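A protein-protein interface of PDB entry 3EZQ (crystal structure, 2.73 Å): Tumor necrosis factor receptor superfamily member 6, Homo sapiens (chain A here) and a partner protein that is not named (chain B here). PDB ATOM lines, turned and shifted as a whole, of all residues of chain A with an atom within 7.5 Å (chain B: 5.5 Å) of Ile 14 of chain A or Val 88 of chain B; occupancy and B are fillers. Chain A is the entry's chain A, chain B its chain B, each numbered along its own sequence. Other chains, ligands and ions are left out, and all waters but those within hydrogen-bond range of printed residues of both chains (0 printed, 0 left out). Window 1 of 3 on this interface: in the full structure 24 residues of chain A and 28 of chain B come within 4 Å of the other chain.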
ATOM      1  N   SER A   8     -21.056  20.655   3.931  1.00  0.00           N
ATOM      2  CA  SER A   8     -22.391  20.392   4.456  1.00  0.00           C
ATOM      3  C   SER A   8     -22.790  18.928   4.312  1.00  0.00           C
ATOM      4  O   SER A   8     -23.344  18.328   5.241  1.00  0.00           O
ATOM      5  CB  SER A   8     -23.458  21.213   3.772  1.00  0.00           C
ATOM      6  OG  SER A   8     -24.727  20.639   4.089  1.00  0.00           O
ATOM      7  N   LYS A   9     -22.538  18.348   3.148  1.00  0.00           N
ATOM      8  CA  LYS A   9     -22.842  16.921   2.969  1.00  0.00           C
ATOM      9  C   LYS A   9     -22.111  16.077   4.002  1.00  0.00           C
ATOM     10  O   LYS A   9     -22.686  15.175   4.617  1.00  0.00           O
ATOM     11  CB  LYS A   9     -22.486  16.436   1.569  1.00  0.00           C
ATOM     12  CG  LYS A   9     -23.386  17.024   0.486  1.00  0.00           C
ATOM     13  CD  LYS A   9     -22.990  16.544  -0.896  1.00  0.00           C
ATOM     14  CE  LYS A   9     -24.174  16.705  -1.855  1.00  0.00           C
ATOM     15  NZ  LYS A   9     -23.887  16.205  -3.220  1.00  0.00           N
ATOM     16  N   TYR A  10     -20.838  16.374   4.211  1.00  0.00           N
ATOM     17  CA  TYR A  10     -20.039  15.659   5.216  1.00  0.00           C
ATOM     18  C   TYR A  10     -20.601  15.813   6.618  1.00  0.00           C
ATOM     19  O   TYR A  10     -20.892  14.840   7.266  1.00  0.00           O
ATOM     20  CB  TYR A  10     -18.604  16.162   5.194  1.00  0.00           C
ATOM     21  CG  TYR A  10     -17.754  15.731   6.354  1.00  0.00           C
ATOM     22  CD1 TYR A  10     -17.700  14.403   6.742  1.00  0.00           C
ATOM     23  CD2 TYR A  10     -16.957  16.646   7.029  1.00  0.00           C
ATOM     24  CE1 TYR A  10     -16.905  14.004   7.783  1.00  0.00           C
ATOM     25  CE2 TYR A  10     -16.148  16.247   8.076  1.00  0.00           C
ATOM     26  CZ  TYR A  10     -16.127  14.924   8.447  1.00  0.00           C
ATOM     27  OH  TYR A  10     -15.343  14.513   9.498  1.00  0.00           O
ATOM     28  N   ILE A  11     -20.755  17.040   7.093  1.00  0.00           N
ATOM     29  CA  ILE A  11     -21.263  17.251   8.457  1.00  0.00           C
ATOM     30  C   ILE A  11     -22.676  16.725   8.636  1.00  0.00           C
ATOM     31  O   ILE A  11     -23.049  16.340   9.721  1.00  0.00           O
ATOM     32  CB  ILE A  11     -21.195  18.727   8.869  1.00  0.00           C
ATOM     33  CG1 ILE A  11     -19.787  19.036   9.382  1.00  0.00           C
ATOM     34  CG2 ILE A  11     -22.224  19.042   9.948  1.00  0.00           C
ATOM     35  CD1 ILE A  11     -19.427  20.489   9.300  1.00  0.00           C
ATOM     36  N   THR A  12     -23.479  16.733   7.580  1.00  0.00           N
ATOM     37  CA  THR A  12     -24.796  16.112   7.656  1.00  0.00           C
ATOM     38  C   THR A  12     -24.647  14.616   7.891  1.00  0.00           C
ATOM     39  O   THR A  12     -25.353  14.034   8.713  1.00  0.00           O
ATOM     40  CB  THR A  12     -25.622  16.350   6.395  1.00  0.00           C
ATOM     41  OG1 THR A  12     -26.055  17.717   6.380  1.00  0.00           O
ATOM     42  CG2 THR A  12     -26.830  15.433   6.360  1.00  0.00           C
ATOM     43  N   THR A  13     -23.717  13.990   7.186  1.00  0.00           N
ATOM     44  CA  THR A  13     -23.498  12.568   7.383  1.00  0.00           C
ATOM     45  C   THR A  13     -23.094  12.230   8.828  1.00  0.00           C
ATOM     46  O   THR A  13     -23.626  11.269   9.407  1.00  0.00           O
ATOM     47  CB  THR A  13     -22.444  12.008   6.444  1.00  0.00           C
ATOM     48  OG1 THR A  13     -22.867  12.217   5.092  1.00  0.00           O
ATOM     49  CG2 THR A  13     -22.246  10.545   6.687  1.00  0.00           C
ATOM     50  N   ILE A  14     -22.188  13.007   9.422  1.00  0.00           N
ATOM     51  CA  ILE A  14     -21.869  12.800  10.834  1.00  0.00           C
ATOM     52  C   ILE A  14     -23.085  13.073  11.709  1.00  0.00           C
ATOM     53  O   ILE A  14     -23.363  12.307  12.617  1.00  0.00           O
ATOM     54  CB  ILE A  14     -20.723  13.680  11.350  1.00  0.00           C
ATOM     55  CG1 ILE A  14     -19.400  13.360  10.626  1.00  0.00           C
ATOM     56  CG2 ILE A  14     -20.569  13.499  12.841  1.00  0.00           C
ATOM     57  CD1 ILE A  14     -19.002  11.896  10.564  1.00  0.00           C
ATOM     58  N   ALA A  15     -23.808  14.158  11.453  1.00  0.00           N
ATOM     59  CA  ALA A  15     -25.000  14.464  12.268  1.00  0.00           C
ATOM     60  C   ALA A  15     -25.976  13.278  12.308  1.00  0.00           C
ATOM     61  O   ALA A  15     -26.588  12.980  13.326  1.00  0.00           O
ATOM     62  CB  ALA A  15     -25.711  15.694  11.745  1.00  0.00           C
ATOM     63  N   GLY A  16     -26.108  12.605  11.175  1.00  0.00           N
ATOM     64  CA  GLY A  16     -27.110  11.568  11.020  1.00  0.00           C
ATOM     65  C   GLY A  16     -26.796  10.342  11.834  1.00  0.00           C
ATOM     66  O   GLY A  16     -27.668   9.497  12.068  1.00  0.00           O
ATOM     67  N   VAL A  17     -25.547  10.231  12.280  1.00  0.00           N
ATOM     68  CA  VAL A  17     -25.131   9.060  13.056  1.00  0.00           C
ATOM     69  C   VAL A  17     -24.882   9.425  14.510  1.00  0.00           C
ATOM     70  O   VAL A  17     -24.197   8.692  15.171  1.00  0.00           O
ATOM     71  CB  VAL A  17     -23.827   8.323  12.563  1.00  0.00           C
ATOM     72  CG1 VAL A  17     -23.913   7.890  11.128  1.00  0.00           C
ATOM     73  CG2 VAL A  17     -22.592   9.116  12.851  1.00  0.00           C
ATOM     74  N   MET A  18     -25.407  10.543  14.993  1.00  0.00           N
ATOM     75  CA  MET A  18     -25.287  10.943  16.392  1.00  0.00           C
ATOM     76  C   MET A  18     -26.622  11.550  16.847  1.00  0.00           C
ATOM     77  O   MET A  18     -27.319  12.201  16.068  1.00  0.00           O
ATOM     78  CB  MET A  18     -24.177  12.003  16.609  1.00  0.00           C
ATOM     79  CG  MET A  18     -22.762  11.678  16.090  1.00  0.00           C
ATOM     80  SD  MET A  18     -21.523  13.031  16.262  1.00  0.00           S
ATOM     81  CE  MET A  18     -21.657  13.479  18.002  1.00  0.00           C
ATOM     82  N   THR A  19     -26.957  11.399  18.122  1.00  0.00           N
ATOM     83  CA  THR A  19     -28.167  12.021  18.659  1.00  0.00           C
ATOM     84  C   THR A  19     -27.865  13.446  19.096  1.00  0.00           C
ATOM     85  O   THR A  19     -26.705  13.795  19.308  1.00  0.00           O
ATOM     86  CB  THR A  19     -28.720  11.230  19.846  1.00  0.00           C
ATOM     87  OG1 THR A  19     -27.668  10.988  20.796  1.00  0.00           O
ATOM     88  CG2 THR A  19     -29.322   9.889  19.380  1.00  0.00           C
ATOM     89  N   GLN A  22     -25.948  13.539  22.207  1.00  0.00           N
ATOM     90  CA  GLN A  22     -24.602  13.098  21.918  1.00  0.00           C
ATOM     91  C   GLN A  22     -23.756  14.200  21.229  1.00  0.00           C
ATOM     92  O   GLN A  22     -22.600  14.406  21.593  1.00  0.00           O
ATOM     93  CB  GLN A  22     -24.680  11.841  21.085  1.00  0.00           C
ATOM     94  CG  GLN A  22     -23.375  11.156  20.843  1.00  0.00           C
ATOM     95  CD  GLN A  22     -23.550   9.875  20.017  1.00  0.00           C
ATOM     96  OE1 GLN A  22     -24.647   9.220  20.034  1.00  0.00           O
ATOM     97  NE2 GLN A  22     -22.457   9.506  19.272  1.00  0.00           N
ATOM     98  N   VAL A  23     -24.327  14.921  20.267  1.00  0.00           N
ATOM     99  CA  VAL A  23     -23.601  16.019  19.623  1.00  0.00           C
ATOM    100  C   VAL A  23     -23.314  17.145  20.587  1.00  0.00           C
ATOM    101  O   VAL A  23     -22.218  17.716  20.583  1.00  0.00           O
ATOM    102  CB  VAL A  23     -24.377  16.615  18.473  1.00  0.00           C
ATOM    103  CG1 VAL A  23     -23.676  17.857  17.970  1.00  0.00           C
ATOM    104  CG2 VAL A  23     -24.500  15.585  17.389  1.00  0.00           C
ATOM    105  N   PHE A  26     -20.474  16.119  22.855  1.00  0.00           N
ATOM    106  CA  PHE A  26     -19.200  16.146  22.172  1.00  0.00           C
ATOM    107  C   PHE A  26     -18.650  17.557  21.962  1.00  0.00           C
ATOM    108  O   PHE A  26     -17.516  17.835  22.332  1.00  0.00           O
ATOM    109  CB  PHE A  26     -19.341  15.457  20.836  1.00  0.00           C
ATOM    110  CG  PHE A  26     -18.107  15.490  20.031  1.00  0.00           C
ATOM    111  CD1 PHE A  26     -16.995  14.806  20.454  1.00  0.00           C
ATOM    112  CD2 PHE A  26     -18.062  16.190  18.852  1.00  0.00           C
ATOM    113  CE1 PHE A  26     -15.853  14.812  19.729  1.00  0.00           C
ATOM    114  CE2 PHE A  26     -16.923  16.214  18.115  1.00  0.00           C
ATOM    115  CZ  PHE A  26     -15.803  15.520  18.560  1.00  0.00           C
ATOM    116  N   LYS A  52     -28.055  19.880  15.234  1.00  0.00           N
ATOM    117  CA  LYS A  52     -26.865  19.023  15.201  1.00  0.00           C
ATOM    118  C   LYS A  52     -25.860  19.502  14.159  1.00  0.00           C
ATOM    119  O   LYS A  52     -24.664  19.543  14.430  1.00  0.00           O
ATOM    120  CB  LYS A  52     -27.226  17.551  14.947  1.00  0.00           C
ATOM    121  CG  LYS A  52     -28.178  16.987  15.978  1.00  0.00           C
ATOM    122  CD  LYS A  52     -28.295  15.463  15.953  1.00  0.00           C
ATOM    123  CE  LYS A  52     -28.841  14.910  14.655  1.00  0.00           C
ATOM    124  NZ  LYS A  52     -29.264  13.481  14.862  1.00  0.00           N
ATOM    125  N   VAL A  53     -26.341  19.890  12.984  1.00  0.00           N
ATOM    126  CA  VAL A  53     -25.441  20.330  11.923  1.00  0.00           C
ATOM    127  C   VAL A  53     -24.739  21.640  12.280  1.00  0.00           C
ATOM    128  O   VAL A  53     -23.526  21.760  12.101  1.00  0.00           O
ATOM    129  CB  VAL A  53     -26.157  20.477  10.566  1.00  0.00           C
ATOM    130  CG1 VAL A  53     -25.190  21.124   9.557  1.00  0.00           C
ATOM    131  CG2 VAL A  53     -26.642  19.109  10.062  1.00  0.00           C
ATOM    132  N   LEU A  56     -22.152  20.986  14.996  1.00  0.00           N
ATOM    133  CA  LEU A  56     -20.962  20.376  14.417  1.00  0.00           C
ATOM    134  C   LEU A  56     -20.201  21.356  13.540  1.00  0.00           C
ATOM    135  O   LEU A  56     -18.979  21.337  13.524  1.00  0.00           O
ATOM    136  CB  LEU A  56     -21.326  19.103  13.635  1.00  0.00           C
ATOM    137  CG  LEU A  56     -21.723  17.902  14.510  1.00  0.00           C
ATOM    138  CD1 LEU A  56     -22.319  16.812  13.664  1.00  0.00           C
ATOM    139  CD2 LEU A  56     -20.526  17.401  15.293  1.00  0.00           C
ATOM    140  N   TRP A  59     -18.226  23.547  15.851  1.00  0.00           N
ATOM    141  CA  TRP A  59     -17.110  22.747  16.354  1.00  0.00           C
ATOM    142  C   TRP A  59     -16.043  22.557  15.291  1.00  0.00           C
ATOM    143  O   TRP A  59     -14.859  22.655  15.578  1.00  0.00           O
ATOM    144  CB  TRP A  59     -17.597  21.373  16.826  1.00  0.00           C
ATOM    145  CG  TRP A  59     -16.503  20.341  16.860  1.00  0.00           C
ATOM    146  CD1 TRP A  59     -15.563  20.172  17.843  1.00  0.00           C
ATOM    147  CD2 TRP A  59     -16.214  19.354  15.853  1.00  0.00           C
ATOM    148  NE1 TRP A  59     -14.721  19.135  17.518  1.00  0.00           N
ATOM    149  CE2 TRP A  59     -15.095  18.615  16.304  1.00  0.00           C
ATOM    150  CE3 TRP A  59     -16.793  19.020  14.619  1.00  0.00           C
ATOM    151  CZ2 TRP A  59     -14.539  17.563  15.561  1.00  0.00           C
ATOM    152  CZ3 TRP A  59     -16.242  17.968  13.884  1.00  0.00           C
ATOM    153  CH2 TRP A  59     -15.120  17.259  14.361  1.00  0.00           C
ATOM    154  N   LEU A  72     -13.276  13.250  17.125  1.00  0.00           N
ATOM    155  CA  LEU A  72     -14.498  12.694  16.538  1.00  0.00           C
ATOM    156  C   LEU A  72     -14.444  11.165  16.413  1.00  0.00           C
ATOM    157  O   LEU A  72     -15.418  10.480  16.730  1.00  0.00           O
ATOM    158  CB  LEU A  72     -14.775  13.305  15.159  1.00  0.00           C
ATOM    159  CG  LEU A  72     -16.070  12.849  14.483  1.00  0.00           C
ATOM    160  CD1 LEU A  72     -17.253  13.284  15.309  1.00  0.00           C
ATOM    161  CD2 LEU A  72     -16.179  13.355  13.075  1.00  0.00           C
ATOM    162  N   LEU A  76     -17.050   8.591  18.182  1.00  0.00           N
ATOM    163  CA  LEU A  76     -17.887   7.630  17.456  1.00  0.00           C
ATOM    164  C   LEU A  76     -17.559   6.192  17.888  1.00  0.00           C
ATOM    165  O   LEU A  76     -18.460   5.348  18.056  1.00  0.00           O
ATOM    166  CB  LEU A  76     -17.719   7.796  15.931  1.00  0.00           C
ATOM    167  CG  LEU A  76     -18.270   9.102  15.336  1.00  0.00           C
ATOM    168  CD1 LEU A  76     -17.818   9.269  13.903  1.00  0.00           C
ATOM    169  CD2 LEU A  76     -19.784   9.205  15.417  1.00  0.00           C
ATOM    170  N   LYS A  77     -16.276   5.923  18.091  1.00  0.00           N
ATOM    171  CA  LYS A  77     -15.807   4.616  18.535  1.00  0.00           C
ATOM    172  C   LYS A  77     -16.485   4.215  19.845  1.00  0.00           C
ATOM    173  O   LYS A  77     -17.051   3.130  19.958  1.00  0.00           O
ATOM    174  CB  LYS A  77     -14.288   4.670  18.735  1.00  0.00           C
ATOM    175  CG  LYS A  77     -13.626   3.350  19.042  1.00  0.00           C
ATOM    176  CD  LYS A  77     -12.210   3.553  19.571  1.00  0.00           C
ATOM    177  CE  LYS A  77     -11.551   2.242  19.943  1.00  0.00           C
ATOM    178  NZ  LYS A  77     -10.216   2.498  20.529  1.00  0.00           N
ATOM    179  N   ASN A  80     -20.243   3.772  19.365  1.00  0.00           N
ATOM    180  CA  ASN A  80     -20.450   2.486  18.695  1.00  0.00           C
ATOM    181  C   ASN A  80     -20.270   1.320  19.638  1.00  0.00           C
ATOM    182  O   ASN A  80     -21.098   0.409  19.676  1.00  0.00           O
ATOM    183  CB  ASN A  80     -19.494   2.328  17.522  1.00  0.00           C
ATOM    184  CG  ASN A  80     -19.888   3.178  16.360  1.00  0.00           C
ATOM    185  OD1 ASN A  80     -21.018   3.669  16.312  1.00  0.00           O
ATOM    186  ND2 ASN A  80     -18.964   3.379  15.415  1.00  0.00           N
ATOM    187  N   GLU A 115     -20.113  -4.406   6.751  1.00  0.00           N
ATOM    188  CA  GLU A 115     -19.218  -3.414   6.158  1.00  0.00           C
ATOM    189  C   GLU A 115     -18.907  -3.685   4.701  1.00  0.00           C
ATOM    190  O   GLU A 115     -18.476  -4.728   4.247  1.00  0.00           O
ATOM    191  CB  GLU A 115     -17.911  -3.316   6.971  1.00  0.00           C
ATOM    192  CG  GLU A 115     -16.833  -2.439   6.310  1.00  0.00           C
ATOM    193  CD  GLU A 115     -15.785  -1.939   7.286  1.00  0.00           C
ATOM    194  OE1 GLU A 115     -16.151  -1.118   8.166  1.00  0.00           O
ATOM    195  OE2 GLU A 115     -14.605  -2.358   7.162  1.00  0.00           O
ATOM    196  OXT GLU A 115     -19.099  -2.771   3.899  1.00  0.00           O
ATOM    197  N   ALA B   7     -22.598   7.738   2.370  1.00  0.00           N
ATOM    198  CA  ALA B   7     -22.039   8.201   3.624  1.00  0.00           C
ATOM    199  C   ALA B   7     -20.517   8.160   3.540  1.00  0.00           C
ATOM    200  O   ALA B   7     -19.854   9.158   3.807  1.00  0.00           O
ATOM    201  CB  ALA B   7     -22.554   7.362   4.761  1.00  0.00           C
ATOM    202  N   VAL B  11     -17.643  11.377   3.548  1.00  0.00           N
ATOM    203  CA  VAL B  11     -16.538  11.465   4.487  1.00  0.00           C
ATOM    204  C   VAL B  11     -15.220  11.583   3.723  1.00  0.00           C
ATOM    205  O   VAL B  11     -14.386  12.419   4.058  1.00  0.00           O
ATOM    206  CB  VAL B  11     -16.495  10.255   5.439  1.00  0.00           C
ATOM    207  CG1 VAL B  11     -15.167  10.207   6.168  1.00  0.00           C
ATOM    208  CG2 VAL B  11     -17.654  10.314   6.416  1.00  0.00           C
ATOM    209  N   ASP B  83     -10.302   5.124   9.354  1.00  0.00           N
ATOM    210  CA  ASP B  83     -10.879   5.030  10.683  1.00  0.00           C
ATOM    211  C   ASP B  83     -12.250   5.690  10.713  1.00  0.00           C
ATOM    212  O   ASP B  83     -13.231   5.081  11.141  1.00  0.00           O
ATOM    213  CB  ASP B  83      -9.972   5.696  11.736  1.00  0.00           C
ATOM    214  CG  ASP B  83      -8.627   5.016  11.877  1.00  0.00           C
ATOM    215  OD1 ASP B  83      -8.501   3.841  11.504  1.00  0.00           O
ATOM    216  OD2 ASP B  83      -7.681   5.666  12.360  1.00  0.00           O
ATOM    217  N   LEU B  84     -12.322   6.932  10.251  1.00  0.00           N
ATOM    218  CA  LEU B  84     -13.570   7.675  10.302  1.00  0.00           C
ATOM    219  C   LEU B  84     -14.664   7.005   9.431  1.00  0.00           C
ATOM    220  O   LEU B  84     -15.820   6.904   9.854  1.00  0.00           O
ATOM    221  CB  LEU B  84     -13.332   9.134   9.912  1.00  0.00           C
ATOM    222  CG  LEU B  84     -14.496  10.118  10.096  1.00  0.00           C
ATOM    223  CD1 LEU B  84     -15.212   9.895  11.433  1.00  0.00           C
ATOM    224  CD2 LEU B  84     -14.018  11.573   9.958  1.00  0.00           C
ATOM    225  N   VAL B  85     -14.299   6.509   8.250  1.00  0.00           N
ATOM    226  CA  VAL B  85     -15.254   5.800   7.401  1.00  0.00           C
ATOM    227  C   VAL B  85     -15.767   4.547   8.099  1.00  0.00           C
ATOM    228  O   VAL B  85     -16.957   4.257   8.050  1.00  0.00           O
ATOM    229  CB  VAL B  85     -14.659   5.450   6.038  1.00  0.00           C
ATOM    230  CG1 VAL B  85     -15.598   4.524   5.281  1.00  0.00           C
ATOM    231  CG2 VAL B  85     -14.383   6.728   5.256  1.00  0.00           C
ATOM    232  N   GLN B  86     -14.873   3.818   8.761  1.00  0.00           N
ATOM    233  CA  GLN B  86     -15.259   2.616   9.475  1.00  0.00           C
ATOM    234  C   GLN B  86     -16.249   2.953  10.586  1.00  0.00           C
ATOM    235  O   GLN B  86     -17.308   2.304  10.695  1.00  0.00           O
ATOM    236  CB  GLN B  86     -14.042   1.917  10.080  1.00  0.00           C
ATOM    237  CG  GLN B  86     -13.248   1.045   9.103  1.00  0.00           C
ATOM    238  CD  GLN B  86     -12.375  -0.037   9.804  1.00  0.00           C
ATOM    239  OE1 GLN B  86     -12.291  -0.103  11.047  1.00  0.00           O
ATOM    240  NE2 GLN B  86     -11.731  -0.890   8.991  1.00  0.00           N
ATOM    241  N   GLU B  87     -15.911   3.951  11.406  1.00  0.00           N
ATOM    242  CA  GLU B  87     -16.761   4.297  12.536  1.00  0.00           C
ATOM    243  C   GLU B  87     -18.124   4.787  12.051  1.00  0.00           C
ATOM    244  O   GLU B  87     -19.137   4.507  12.691  1.00  0.00           O
ATOM    245  CB  GLU B  87     -16.148   5.380  13.430  1.00  0.00           C
ATOM    246  CG  GLU B  87     -14.801   5.088  14.098  1.00  0.00           C
ATOM    247  CD  GLU B  87     -14.789   3.853  14.983  1.00  0.00           C
ATOM    248  OE1 GLU B  87     -15.875   3.376  15.369  1.00  0.00           O
ATOM    249  OE2 GLU B  87     -13.676   3.359  15.293  1.00  0.00           O
ATOM    250  N   VAL B  88     -18.173   5.511  10.932  1.00  0.00           N
ATOM    251  CA  VAL B  88     -19.477   5.971  10.426  1.00  0.00           C
ATOM    252  C   VAL B  88     -20.275   4.773   9.933  1.00  0.00           C
ATOM    253  O   VAL B  88     -21.463   4.634  10.227  1.00  0.00           O
ATOM    254  CB  VAL B  88     -19.386   6.999   9.330  1.00  0.00           C
ATOM    255  CG1 VAL B  88     -20.746   7.117   8.640  1.00  0.00           C
ATOM    256  CG2 VAL B  88     -18.955   8.344   9.917  1.00  0.00           C
ATOM    257  N   GLN B  89     -19.606   3.871   9.230  1.00  0.00           N
ATOM    258  CA  GLN B  89     -20.277   2.670   8.758  1.00  0.00           C
ATOM    259  C   GLN B  89     -20.798   1.858   9.941  1.00  0.00           C
ATOM    260  O   GLN B  89     -21.908   1.328   9.886  1.00  0.00           O
ATOM    261  CB  GLN B  89     -19.319   1.829   7.906  1.00  0.00           C
ATOM    262  CG  GLN B  89     -19.894   0.524   7.408  1.00  0.00           C
ATOM    263  CD  GLN B  89     -21.096   0.751   6.542  1.00  0.00           C
ATOM    264  OE1 GLN B  89     -21.038   1.539   5.598  1.00  0.00           O
ATOM    265  NE2 GLN B  89     -22.204   0.084   6.859  1.00  0.00           N
ATOM    266  N   GLN B  90     -19.996   1.746  10.996  1.00  0.00           N
ATOM    267  CA  GLN B  90     -20.395   0.953  12.149  1.00  0.00           C
ATOM    268  C   GLN B  90     -21.575   1.620  12.839  1.00  0.00           C
ATOM    269  O   GLN B  90     -22.512   0.924  13.263  1.00  0.00           O
ATOM    270  CB  GLN B  90     -19.233   0.759  13.114  1.00  0.00           C
ATOM    271  CG  GLN B  90     -19.603   0.031  14.370  1.00  0.00           C
ATOM    272  CD  GLN B  90     -20.058  -1.362  14.087  1.00  0.00           C
ATOM    273  OE1 GLN B  90     -19.258  -2.224  13.760  1.00  0.00           O
ATOM    274  NE2 GLN B  90     -21.350  -1.595  14.190  1.00  0.00           N
ATOM    275  N   ALA B  91     -21.516   2.948  12.958  1.00  0.00           N
ATOM    276  CA  ALA B  91     -22.616   3.713  13.521  1.00  0.00           C
ATOM    277  C   ALA B  91     -23.872   3.408  12.720  1.00  0.00           C
ATOM    278  O   ALA B  91     -24.924   3.114  13.287  1.00  0.00           O
ATOM    279  CB  ALA B  91     -22.311   5.228  13.517  1.00  0.00           C
ATOM    280  N   ARG B  92     -23.758   3.452  11.404  1.00  0.00           N
ATOM    281  CA  ARG B  92     -24.925   3.213  10.553  1.00  0.00           C
ATOM    282  C   ARG B  92     -25.503   1.813  10.727  1.00  0.00           C
ATOM    283  O   ARG B  92     -26.730   1.643  10.724  1.00  0.00           O
ATOM    284  CB  ARG B  92     -24.581   3.447   9.097  1.00  0.00           C
ATOM    285  CG  ARG B  92     -24.359   4.888   8.788  1.00  0.00           C
ATOM    286  CD  ARG B  92     -23.860   5.029   7.377  1.00  0.00           C
ATOM    287  NE  ARG B  92     -24.896   4.678   6.398  1.00  0.00           N
ATOM    288  CZ  ARG B  92     -25.928   5.454   6.087  1.00  0.00           C
ATOM    289  NH1 ARG B  92     -26.102   6.635   6.676  1.00  0.00           N
ATOM    290  NH2 ARG B  92     -26.803   5.039   5.185  1.00  0.00           N
ATOM    291  N   ASP B  93     -24.634   0.821  10.908  1.00  0.00           N
ATOM    292  CA  ASP B  93     -25.101  -0.533  11.177  1.00  0.00           C
ATOM    293  C   ASP B  93     -25.944  -0.621  12.434  1.00  0.00           C
ATOM    294  O   ASP B  93     -26.802  -1.474  12.546  1.00  0.00           O
ATOM    295  CB  ASP B  93     -23.935  -1.496  11.309  1.00  0.00           C
ATOM    296  CG  ASP B  93     -23.179  -1.694  10.020  1.00  0.00           C
ATOM    297  OD1 ASP B  93     -23.701  -1.364   8.948  1.00  0.00           O
ATOM    298  OD2 ASP B  93     -22.048  -2.212  10.091  1.00  0.00           O
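Printed residues of chain B within 4 Å of Leu 76 of chain A: Leu 84 (3.6 Å) and Glu 87 (3.8 Å).
Printed residues of chain A within 4 Å of Ala 7 of chain B: Thr 13.
Printed residues of chain A within 4 Å of Leu 84 of chain B: Tyr 10 (3.3 Å), Leu 72 (3.95 Å) and Leu 76 (3.6 Å).
Val 88 of chain B touches just one residue of chain A: Ile 14.
The nearest printed residue of chain B that does not touch Asn 80 of chain A is Val 88 of chain B (5.0 Å).
ND2 of Asn 80 of chain A is in hydrogen-bond range of O of Glu 87 of chain B.
The backbone NH (N) of Ala 91 of chain B sits close to the side-chain amide oxygen (OD1) of Asn 80 of chain A (3.5 Å).
The backbone carbonyl oxygen of Lys 9 of chain A is in hydrogen-bond range of the side-chain hydroxyl of Thr 13 of chain A, 3.0 Å away.
The backbone carbonyl oxygen of Leu 76 of chain A lies close to the side-chain amide nitrogen of Asn 80 of chain A (3.3 Å).
Of the 13 printed residues of chain B, 9 touch a printed residue of chain A.
Hydrophobic or aromatic side chains of chain A that line the printed part of chain B: Tyr 10, Ile 14, Val 17, Leu 72 and Leu 76.
Among the printed residues, no Asp or Glu carboxylate lies within 4 Å of a Lys or Arg side-chain nitrogen of the other chain.
Among the printed residues, merely in contact across the chains: Tyr 10 of chain A with Val 11 of chain B (3.9 Å), Tyr 10 of chain A with Leu 84 of chain B (3.3 Å), Thr 13 of chain A with Ala 7 of chain B (3.7 Å), Ile 14 of chain A with Val 88 of chain B (3.6 Å), Val 17 of chain A with Ala 91 of chain B (3.6 Å), Val 17 of chain A with Arg 92 of chain B (3.8 Å), Leu 72 of chain A with Leu 84 of chain B (3.95 Å), Leu 76 of chain A with Leu 84 of chain B (3.6 Å), Leu 76 of chain A with Glu 87 of chain B (3.8 Å), Lys 77 of chain A with Glu 87 of chain B (3.4 Å), Asn 80 of chain A with Gln 90 of chain B (3.5 Å) and Glu 115 of chain A with Gln 86 of chain B (3.7 Å).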
